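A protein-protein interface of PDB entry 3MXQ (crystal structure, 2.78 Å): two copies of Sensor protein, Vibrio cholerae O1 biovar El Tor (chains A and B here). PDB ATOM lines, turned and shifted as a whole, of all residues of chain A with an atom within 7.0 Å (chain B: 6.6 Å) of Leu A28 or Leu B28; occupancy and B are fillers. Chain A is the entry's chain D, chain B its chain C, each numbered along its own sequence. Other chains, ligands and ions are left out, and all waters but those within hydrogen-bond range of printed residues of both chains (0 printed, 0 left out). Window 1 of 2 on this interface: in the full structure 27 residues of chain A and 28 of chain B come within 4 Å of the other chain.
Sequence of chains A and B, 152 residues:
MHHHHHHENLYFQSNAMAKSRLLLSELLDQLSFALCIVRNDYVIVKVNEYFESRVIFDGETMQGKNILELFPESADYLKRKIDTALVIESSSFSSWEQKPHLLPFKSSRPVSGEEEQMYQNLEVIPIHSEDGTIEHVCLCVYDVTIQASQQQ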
ATOM      1  N   LEU A  22      25.185   1.555   8.042  1.00  0.00           N
ATOM      2  CA  LEU A  22      24.519   1.038   9.233  1.00  0.00           C
ATOM      3  C   LEU A  22      23.123   0.451   8.966  1.00  0.00           C
ATOM      4  O   LEU A  22      22.819  -0.683   9.396  1.00  0.00           O
ATOM      5  CB  LEU A  22      24.462   2.093  10.333  1.00  0.00           C
ATOM      6  CG  LEU A  22      25.786   2.333  11.044  1.00  0.00           C
ATOM      7  CD1 LEU A  22      25.793   3.682  11.743  1.00  0.00           C
ATOM      8  CD2 LEU A  22      26.082   1.203  12.009  1.00  0.00           C
ATOM      9  N   LEU A  23      22.289   1.206   8.248  1.00  0.00           N
ATOM     10  CA  LEU A  23      20.946   0.740   7.873  1.00  0.00           C
ATOM     11  C   LEU A  23      20.968  -0.558   7.059  1.00  0.00           C
ATOM     12  O   LEU A  23      20.181  -1.486   7.324  1.00  0.00           O
ATOM     13  CB  LEU A  23      20.197   1.825   7.105  1.00  0.00           C
ATOM     14  CG  LEU A  23      19.739   3.052   7.899  1.00  0.00           C
ATOM     15  CD1 LEU A  23      18.917   3.945   7.015  1.00  0.00           C
ATOM     16  CD2 LEU A  23      18.922   2.657   9.135  1.00  0.00           C
ATOM     17  N   LEU A  24      21.872  -0.626   6.076  1.00  0.00           N
ATOM     18  CA  LEU A  24      22.004  -1.822   5.249  1.00  0.00           C
ATOM     19  C   LEU A  24      22.407  -3.003   6.106  1.00  0.00           C
ATOM     20  O   LEU A  24      21.955  -4.125   5.899  1.00  0.00           O
ATOM     21  CB  LEU A  24      23.034  -1.626   4.143  1.00  0.00           C
ATOM     22  CG  LEU A  24      23.170  -2.852   3.229  1.00  0.00           C
ATOM     23  CD1 LEU A  24      21.837  -3.228   2.582  1.00  0.00           C
ATOM     24  CD2 LEU A  24      24.260  -2.677   2.180  1.00  0.00           C
ATOM     25  N   SER A  25      23.261  -2.737   7.081  1.00  0.00           N
ATOM     26  CA  SER A  25      23.725  -3.778   7.953  1.00  0.00           C
ATOM     27  C   SER A  25      22.546  -4.306   8.788  1.00  0.00           C
ATOM     28  O   SER A  25      22.485  -5.505   9.094  1.00  0.00           O
ATOM     29  CB  SER A  25      24.856  -3.254   8.837  1.00  0.00           C
ATOM     30  OG  SER A  25      25.290  -4.244   9.756  1.00  0.00           O
ATOM     31  N   GLU A  26      21.612  -3.418   9.142  1.00  0.00           N
ATOM     32  CA  GLU A  26      20.476  -3.812   9.974  1.00  0.00           C
ATOM     33  C   GLU A  26      19.467  -4.616   9.138  1.00  0.00           C
ATOM     34  O   GLU A  26      19.046  -5.717   9.527  1.00  0.00           O
ATOM     35  CB  GLU A  26      19.841  -2.594  10.631  1.00  0.00           C
ATOM     36  CG  GLU A  26      18.802  -2.931  11.696  1.00  0.00           C
ATOM     37  CD  GLU A  26      18.104  -1.689  12.298  1.00  0.00           C
ATOM     38  OE1 GLU A  26      17.177  -1.891  13.130  1.00  0.00           O
ATOM     39  OE2 GLU A  26      18.476  -0.528  11.962  1.00  0.00           O
ATOM     40  N   LEU A  27      19.129  -4.076   7.968  1.00  0.00           N
ATOM     41  CA  LEU A  27      18.299  -4.771   6.997  1.00  0.00           C
ATOM     42  C   LEU A  27      18.831  -6.164   6.709  1.00  0.00           C
ATOM     43  O   LEU A  27      18.081  -7.121   6.820  1.00  0.00           O
ATOM     44  CB  LEU A  27      18.201  -3.967   5.695  1.00  0.00           C
ATOM     45  CG  LEU A  27      17.392  -4.625   4.578  1.00  0.00           C
ATOM     46  CD1 LEU A  27      15.968  -4.806   5.023  1.00  0.00           C
ATOM     47  CD2 LEU A  27      17.434  -3.833   3.306  1.00  0.00           C
ATOM     48  N   LEU A  28      20.109  -6.282   6.341  1.00  0.00           N
ATOM     49  CA  LEU A  28      20.689  -7.600   6.064  1.00  0.00           C
ATOM     50  C   LEU A  28      20.659  -8.530   7.258  1.00  0.00           C
ATOM     51  O   LEU A  28      20.365  -9.702   7.108  1.00  0.00           O
ATOM     52  CB  LEU A  28      22.122  -7.511   5.569  1.00  0.00           C
ATOM     53  CG  LEU A  28      22.325  -6.844   4.222  1.00  0.00           C
ATOM     54  CD1 LEU A  28      23.805  -6.885   3.865  1.00  0.00           C
ATOM     55  CD2 LEU A  28      21.457  -7.498   3.157  1.00  0.00           C
ATOM     56  N   ASP A  29      20.959  -8.013   8.441  1.00  0.00           N
ATOM     57  CA  ASP A  29      20.964  -8.865   9.613  1.00  0.00           C
ATOM     58  C   ASP A  29      19.537  -9.325  10.011  1.00  0.00           C
ATOM     59  O   ASP A  29      19.376 -10.387  10.598  1.00  0.00           O
ATOM     60  CB  ASP A  29      21.731  -8.208  10.770  1.00  0.00           C
ATOM     61  CG  ASP A  29      23.284  -8.148  10.530  1.00  0.00           C
ATOM     62  OD1 ASP A  29      23.760  -7.622   9.472  1.00  0.00           O
ATOM     63  OD2 ASP A  29      24.039  -8.596  11.436  1.00  0.00           O
ATOM     64  N   GLN A  30      18.519  -8.542   9.649  1.00  0.00           N
ATOM     65  CA  GLN A  30      17.114  -8.879   9.902  1.00  0.00           C
ATOM     66  C   GLN A  30      16.631 -10.009   9.011  1.00  0.00           C
ATOM     67  O   GLN A  30      15.934 -10.905   9.479  1.00  0.00           O
ATOM     68  CB  GLN A  30      16.205  -7.669   9.663  1.00  0.00           C
ATOM     69  CG  GLN A  30      16.204  -6.604  10.764  1.00  0.00           C
ATOM     70  CD  GLN A  30      15.105  -6.814  11.788  1.00  0.00           C
ATOM     71  OE1 GLN A  30      14.001  -7.262  11.453  1.00  0.00           O
ATOM     72  NE2 GLN A  30      15.401  -6.501  13.049  1.00  0.00           N
ATOM     73  N   LEU A  31      16.985  -9.962   7.729  1.00  0.00           N
ATOM     74  CA  LEU A  31      16.512 -10.946   6.751  1.00  0.00           C
ATOM     75  C   LEU A  31      17.353 -12.208   6.697  1.00  0.00           C
ATOM     76  O   LEU A  31      16.918 -13.217   6.165  1.00  0.00           O
ATOM     77  CB  LEU A  31      16.474 -10.333   5.370  1.00  0.00           C
ATOM     78  CG  LEU A  31      15.603  -9.094   5.238  1.00  0.00           C
ATOM     79  CD1 LEU A  31      16.127  -8.271   4.086  1.00  0.00           C
ATOM     80  CD2 LEU A  31      14.155  -9.490   5.040  1.00  0.00           C
ATOM     81  N   SER A  32      18.559 -12.132   7.239  1.00  0.00           N
ATOM     82  CA  SER A  32      19.433 -13.274   7.430  1.00  0.00           C
ATOM     83  C   SER A  32      18.657 -14.549   7.796  1.00  0.00           C
ATOM     84  O   SER A  32      17.929 -14.574   8.790  1.00  0.00           O
ATOM     85  CB  SER A  32      20.405 -12.940   8.564  1.00  0.00           C
ATOM     86  OG  SER A  32      19.750 -13.021   9.839  1.00  0.00           O
ATOM     87  N   PHE A  33      18.803 -15.600   6.996  1.00  0.00           N
ATOM     88  CA  PHE A  33      18.174 -16.893   7.322  1.00  0.00           C
ATOM     89  C   PHE A  33      18.983 -18.075   6.798  1.00  0.00           C
ATOM     90  O   PHE A  33      19.811 -17.912   5.909  1.00  0.00           O
ATOM     91  CB  PHE A  33      16.720 -16.961   6.834  1.00  0.00           C
ATOM     92  CG  PHE A  33      16.570 -17.133   5.344  1.00  0.00           C
ATOM     93  CD1 PHE A  33      16.653 -16.037   4.488  1.00  0.00           C
ATOM     94  CD2 PHE A  33      16.311 -18.397   4.798  1.00  0.00           C
ATOM     95  CE1 PHE A  33      16.492 -16.198   3.112  1.00  0.00           C
ATOM     96  CE2 PHE A  33      16.147 -18.572   3.418  1.00  0.00           C
ATOM     97  CZ  PHE A  33      16.240 -17.479   2.577  1.00  0.00           C
ATOM     98  N   TYR A  50      25.398 -18.726   5.037  1.00  0.00           N
ATOM     99  CA  TYR A  50      24.852 -18.423   6.352  1.00  0.00           C
ATOM    100  C   TYR A  50      24.704 -19.655   7.233  1.00  0.00           C
ATOM    101  O   TYR A  50      25.046 -19.619   8.411  1.00  0.00           O
ATOM    102  CB  TYR A  50      23.506 -17.732   6.209  1.00  0.00           C
ATOM    103  CG  TYR A  50      22.909 -17.238   7.504  1.00  0.00           C
ATOM    104  CD1 TYR A  50      21.928 -17.970   8.168  1.00  0.00           C
ATOM    105  CD2 TYR A  50      23.314 -16.029   8.063  1.00  0.00           C
ATOM    106  CE1 TYR A  50      21.358 -17.513   9.359  1.00  0.00           C
ATOM    107  CE2 TYR A  50      22.753 -15.560   9.251  1.00  0.00           C
ATOM    108  CZ  TYR A  50      21.777 -16.306   9.892  1.00  0.00           C
ATOM    109  OH  TYR A  50      21.231 -15.846  11.063  1.00  0.00           O
ATOM    110  N   LEU B  23      16.578 -16.887  -4.372  1.00  0.00           N
ATOM    111  CA  LEU B  23      17.038 -15.617  -4.881  1.00  0.00           C
ATOM    112  C   LEU B  23      17.404 -14.721  -3.719  1.00  0.00           C
ATOM    113  O   LEU B  23      18.488 -14.112  -3.698  1.00  0.00           O
ATOM    114  CB  LEU B  23      15.950 -14.956  -5.732  1.00  0.00           C
ATOM    115  CG  LEU B  23      16.251 -13.557  -6.284  1.00  0.00           C
ATOM    116  CD1 LEU B  23      17.671 -13.429  -6.863  1.00  0.00           C
ATOM    117  CD2 LEU B  23      15.221 -13.143  -7.333  1.00  0.00           C
ATOM    118  N   LEU B  24      16.491 -14.634  -2.755  1.00  0.00           N
ATOM    119  CA  LEU B  24      16.693 -13.799  -1.581  1.00  0.00           C
ATOM    120  C   LEU B  24      18.020 -14.169  -0.920  1.00  0.00           C
ATOM    121  O   LEU B  24      18.856 -13.308  -0.629  1.00  0.00           O
ATOM    122  CB  LEU B  24      15.529 -13.995  -0.605  1.00  0.00           C
ATOM    123  CG  LEU B  24      15.550 -13.187   0.702  1.00  0.00           C
ATOM    124  CD1 LEU B  24      16.080 -11.761   0.502  1.00  0.00           C
ATOM    125  CD2 LEU B  24      14.177 -13.182   1.359  1.00  0.00           C
ATOM    126  N   SER B  25      18.201 -15.467  -0.721  1.00  0.00           N
ATOM    127  CA  SER B  25      19.380 -15.995  -0.115  1.00  0.00           C
ATOM    128  C   SER B  25      20.620 -15.584  -0.876  1.00  0.00           C
ATOM    129  O   SER B  25      21.638 -15.315  -0.271  1.00  0.00           O
ATOM    130  CB  SER B  25      19.286 -17.511  -0.066  1.00  0.00           C
ATOM    131  OG  SER B  25      20.480 -18.064   0.433  1.00  0.00           O
ATOM    132  N   GLU B  26      20.542 -15.544  -2.199  1.00  0.00           N
ATOM    133  CA  GLU B  26      21.739 -15.356  -3.000  1.00  0.00           C
ATOM    134  C   GLU B  26      22.101 -13.871  -3.014  1.00  0.00           C
ATOM    135  O   GLU B  26      23.293 -13.518  -3.074  1.00  0.00           O
ATOM    136  CB  GLU B  26      21.552 -15.946  -4.398  1.00  0.00           C
ATOM    137  CG  GLU B  26      22.698 -16.868  -4.838  1.00  0.00           C
ATOM    138  CD  GLU B  26      22.255 -18.310  -5.298  1.00  0.00           C
ATOM    139  OE1 GLU B  26      21.024 -18.601  -5.443  1.00  0.00           O
ATOM    140  OE2 GLU B  26      23.167 -19.166  -5.513  1.00  0.00           O
ATOM    141  N   LEU B  27      21.090 -12.996  -2.928  1.00  0.00           N
ATOM    142  CA  LEU B  27      21.355 -11.567  -2.770  1.00  0.00           C
ATOM    143  C   LEU B  27      21.969 -11.272  -1.394  1.00  0.00           C
ATOM    144  O   LEU B  27      22.915 -10.486  -1.296  1.00  0.00           O
ATOM    145  CB  LEU B  27      20.094 -10.723  -2.951  1.00  0.00           C
ATOM    146  CG  LEU B  27      19.402 -10.656  -4.311  1.00  0.00           C
ATOM    147  CD1 LEU B  27      18.048 -10.026  -4.157  1.00  0.00           C
ATOM    148  CD2 LEU B  27      20.198  -9.886  -5.345  1.00  0.00           C
ATOM    149  N   LEU B  28      21.433 -11.864  -0.327  1.00  0.00           N
ATOM    150  CA  LEU B  28      21.988 -11.569   0.989  1.00  0.00           C
ATOM    151  C   LEU B  28      23.423 -12.063   1.115  1.00  0.00           C
ATOM    152  O   LEU B  28      24.236 -11.420   1.788  1.00  0.00           O
ATOM    153  CB  LEU B  28      21.139 -12.123   2.129  1.00  0.00           C
ATOM    154  CG  LEU B  28      19.663 -11.731   2.198  1.00  0.00           C
ATOM    155  CD1 LEU B  28      18.946 -12.540   3.302  1.00  0.00           C
ATOM    156  CD2 LEU B  28      19.472 -10.208   2.374  1.00  0.00           C
ATOM    157  N   ASP B  29      23.742 -13.187   0.476  1.00  0.00           N
ATOM    158  CA  ASP B  29      25.102 -13.697   0.539  1.00  0.00           C
ATOM    159  C   ASP B  29      26.018 -12.705  -0.191  1.00  0.00           C
ATOM    160  O   ASP B  29      27.102 -12.382   0.290  1.00  0.00           O
ATOM    161  CB  ASP B  29      25.236 -15.120  -0.038  1.00  0.00           C
ATOM    162  CG  ASP B  29      24.708 -16.234   0.925  1.00  0.00           C
ATOM    163  OD1 ASP B  29      23.595 -16.068   1.511  1.00  0.00           O
ATOM    164  OD2 ASP B  29      25.387 -17.299   1.075  1.00  0.00           O
ATOM    165  N   GLN B  30      25.578 -12.188  -1.333  1.00  0.00           N
ATOM    166  CA  GLN B  30      26.434 -11.301  -2.120  1.00  0.00           C
ATOM    167  C   GLN B  30      26.560  -9.871  -1.567  1.00  0.00           C
ATOM    168  O   GLN B  30      27.575  -9.202  -1.778  1.00  0.00           O
ATOM    169  CB  GLN B  30      25.972 -11.284  -3.565  1.00  0.00           C
ATOM    170  CG  GLN B  30      26.785 -12.183  -4.467  1.00  0.00           C
ATOM    171  CD  GLN B  30      26.094 -12.461  -5.790  1.00  0.00           C
ATOM    172  OE1 GLN B  30      24.863 -12.593  -5.856  1.00  0.00           O
ATOM    173  NE2 GLN B  30      26.885 -12.572  -6.851  1.00  0.00           N
ATOM    174  N   LEU B  31      25.533  -9.403  -0.873  1.00  0.00           N
ATOM    175  CA  LEU B  31      25.571  -8.090  -0.242  1.00  0.00           C
ATOM    176  C   LEU B  31      26.118  -8.079   1.174  1.00  0.00           C
ATOM    177  O   LEU B  31      26.304  -7.033   1.735  1.00  0.00           O
ATOM    178  CB  LEU B  31      24.188  -7.441  -0.226  1.00  0.00           C
ATOM    179  CG  LEU B  31      23.512  -7.035  -1.524  1.00  0.00           C
ATOM    180  CD1 LEU B  31      22.020  -7.068  -1.298  1.00  0.00           C
ATOM    181  CD2 LEU B  31      23.931  -5.663  -1.962  1.00  0.00           C
ATOM    182  N   SER B  32      26.375  -9.212   1.782  1.00  0.00           N
ATOM    183  CA  SER B  32      26.795  -9.169   3.181  1.00  0.00           C
ATOM    184  C   SER B  32      28.188  -8.592   3.293  1.00  0.00           C
ATOM    185  O   SER B  32      28.999  -8.777   2.402  1.00  0.00           O
ATOM    186  CB  SER B  32      26.758 -10.555   3.779  1.00  0.00           C
ATOM    187  OG  SER B  32      27.396 -11.453   2.903  1.00  0.00           O
ATOM    188  N   PHE B  33      28.460  -7.872   4.374  1.00  0.00           N
ATOM    189  CA  PHE B  33      29.785  -7.280   4.591  1.00  0.00           C
ATOM    190  C   PHE B  33      30.041  -7.081   6.061  1.00  0.00           C
ATOM    191  O   PHE B  33      29.107  -7.072   6.865  1.00  0.00           O
ATOM    192  CB  PHE B  33      29.908  -5.935   3.885  1.00  0.00           C
ATOM    193  CG  PHE B  33      28.955  -4.888   4.395  1.00  0.00           C
ATOM    194  CD1 PHE B  33      27.639  -4.867   3.984  1.00  0.00           C
ATOM    195  CD2 PHE B  33      29.388  -3.906   5.274  1.00  0.00           C
ATOM    196  CE1 PHE B  33      26.776  -3.886   4.445  1.00  0.00           C
ATOM    197  CE2 PHE B  33      28.523  -2.937   5.740  1.00  0.00           C
ATOM    198  CZ  PHE B  33      27.219  -2.926   5.322  1.00  0.00           C
ATOM    199  N   GLU B  49      26.995  -8.747  12.713  1.00  0.00           N
ATOM    200  CA  GLU B  49      27.017 -10.212  12.718  1.00  0.00           C
ATOM    201  C   GLU B  49      28.083 -10.780  11.777  1.00  0.00           C
ATOM    202  O   GLU B  49      28.756 -11.748  12.138  1.00  0.00           O
ATOM    203  CB  GLU B  49      25.627 -10.812  12.387  1.00  0.00           C
ATOM    204  CG  GLU B  49      24.588 -10.801  13.534  1.00  0.00           C
ATOM    205  CD  GLU B  49      23.209 -11.384  13.125  1.00  0.00           C
ATOM    206  OE1 GLU B  49      22.279 -10.586  12.809  1.00  0.00           O
ATOM    207  OE2 GLU B  49      23.050 -12.639  13.119  1.00  0.00           O
ATOM    208  N   TYR B  50      28.249 -10.191  10.586  1.00  0.00           N
ATOM    209  CA  TYR B  50      29.214 -10.741   9.636  1.00  0.00           C
ATOM    210  C   TYR B  50      30.638 -10.632  10.151  1.00  0.00           C
ATOM    211  O   TYR B  50      31.473 -11.515   9.896  1.00  0.00           O
ATOM    212  CB  TYR B  50      29.064 -10.136   8.255  1.00  0.00           C
ATOM    213  CG  TYR B  50      27.696 -10.413   7.708  1.00  0.00           C
ATOM    214  CD1 TYR B  50      27.308 -11.721   7.366  1.00  0.00           C
ATOM    215  CD2 TYR B  50      26.749  -9.377   7.554  1.00  0.00           C
ATOM    216  CE1 TYR B  50      26.014 -11.992   6.888  1.00  0.00           C
ATOM    217  CE2 TYR B  50      25.461  -9.644   7.070  1.00  0.00           C
ATOM    218  CZ  TYR B  50      25.108 -10.952   6.741  1.00  0.00           C
ATOM    219  OH  TYR B  50      23.852 -11.212   6.251  1.00  0.00           O
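The side-chain carboxylate of Asp A29 lies close to the backbone NH of Glu B49 (3.2 Å).
O of Asp A29 is in hydrogen-bond range of OG of Ser A32.
The backbone carbonyl oxygen (O) of Ser A25 sits close to the side-chain carboxylate (OD1) of Asp A29, at 2.5 Å.
OG of Ser A32 lies within hydrogen-bond range of OH of Tyr A50, at 3.4 Å.
The backbone carbonyl oxygen of Leu B28 sits close to the side-chain hydroxyl of Ser B32, 3.4 Å away.
The backbone carbonyl oxygen of Asp B29 lies within hydrogen-bond range of the side-chain hydroxyl of Ser B32 (2.8 Å).
CE1 of Phe B33 touches CD2 of Leu A24, at 3.6 Å.
Leu A28 touches Leu B28.
Leu A28 touches Leu B31 (CD1 to O, 3.3 Å).
Ser B32 touches Leu A28 (CA to CD1, 3.8 Å).
Leu A28 touches Tyr B50 (O to OH, 3.9 Å).
Tyr B50 touches Asp A29 (CE2 to OD1, 3.6 Å).
Leu A31 touches Leu B28.
N of Ser A32 touches CD1 of Leu B28, at 3.98 Å.
Phe A33 touches Leu B24 (CE1 to CG, 3.97 Å).
Of the printed residues of chain B, Leu A24 touches Phe B33.
Leu A28 touches just these residues of chain B: Leu B28 (3.4 Å), Leu B31 (3.3 Å), Ser B32 (3.8 Å) and Tyr B50 (3.9 Å).
Of the printed residues of chain B, Leu A31 touches Leu B28.
Leu B23 touches none of the printed residues of chain A.
Of chain A, only Leu A28, Leu A31 and Ser A32 come within 4 Å of Leu B28.
Of the printed residues of chain A, Leu B31 touches Leu A28.
The nearest residue of chain A that does not touch Leu B28 is Phe A33 (4.3 Å).
The nearest printed residue of chain A that does not touch Leu B24 is Leu A31 (5.0 Å).
Hydrophobic or aromatic side chains of chain A within 4 Å of the printed part of chain B: Leu A24, Leu A28, Leu A31 and Phe A33.
Of the 13 printed residues of chain B, 7 touch a printed residue of chain A.
Hydrophobic or aromatic side chains of chain B within 4 Å of the printed part of chain A: Leu B24, Leu B28, Phe B33 and Tyr B50.
Leu A24 touches Phe B33, and with the chains exchanged Phe A33 touches Leu B24.
Leu A28 touches Ser B32, and with the chains exchanged Ser A32 touches Leu B28.
Leu A28 touches Tyr B50, but with the chains exchanged Tyr A50 does not touch Leu B28 (7.3 Å).
Asp A29 touches Tyr B50, but with the chains exchanged Tyr A50 does not touch Asp B29 (4.2 Å).
Positions printed for both chains: 23, 24, 25, 26, 27, 28, 29, 30, 31, 32, 33 and 50.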
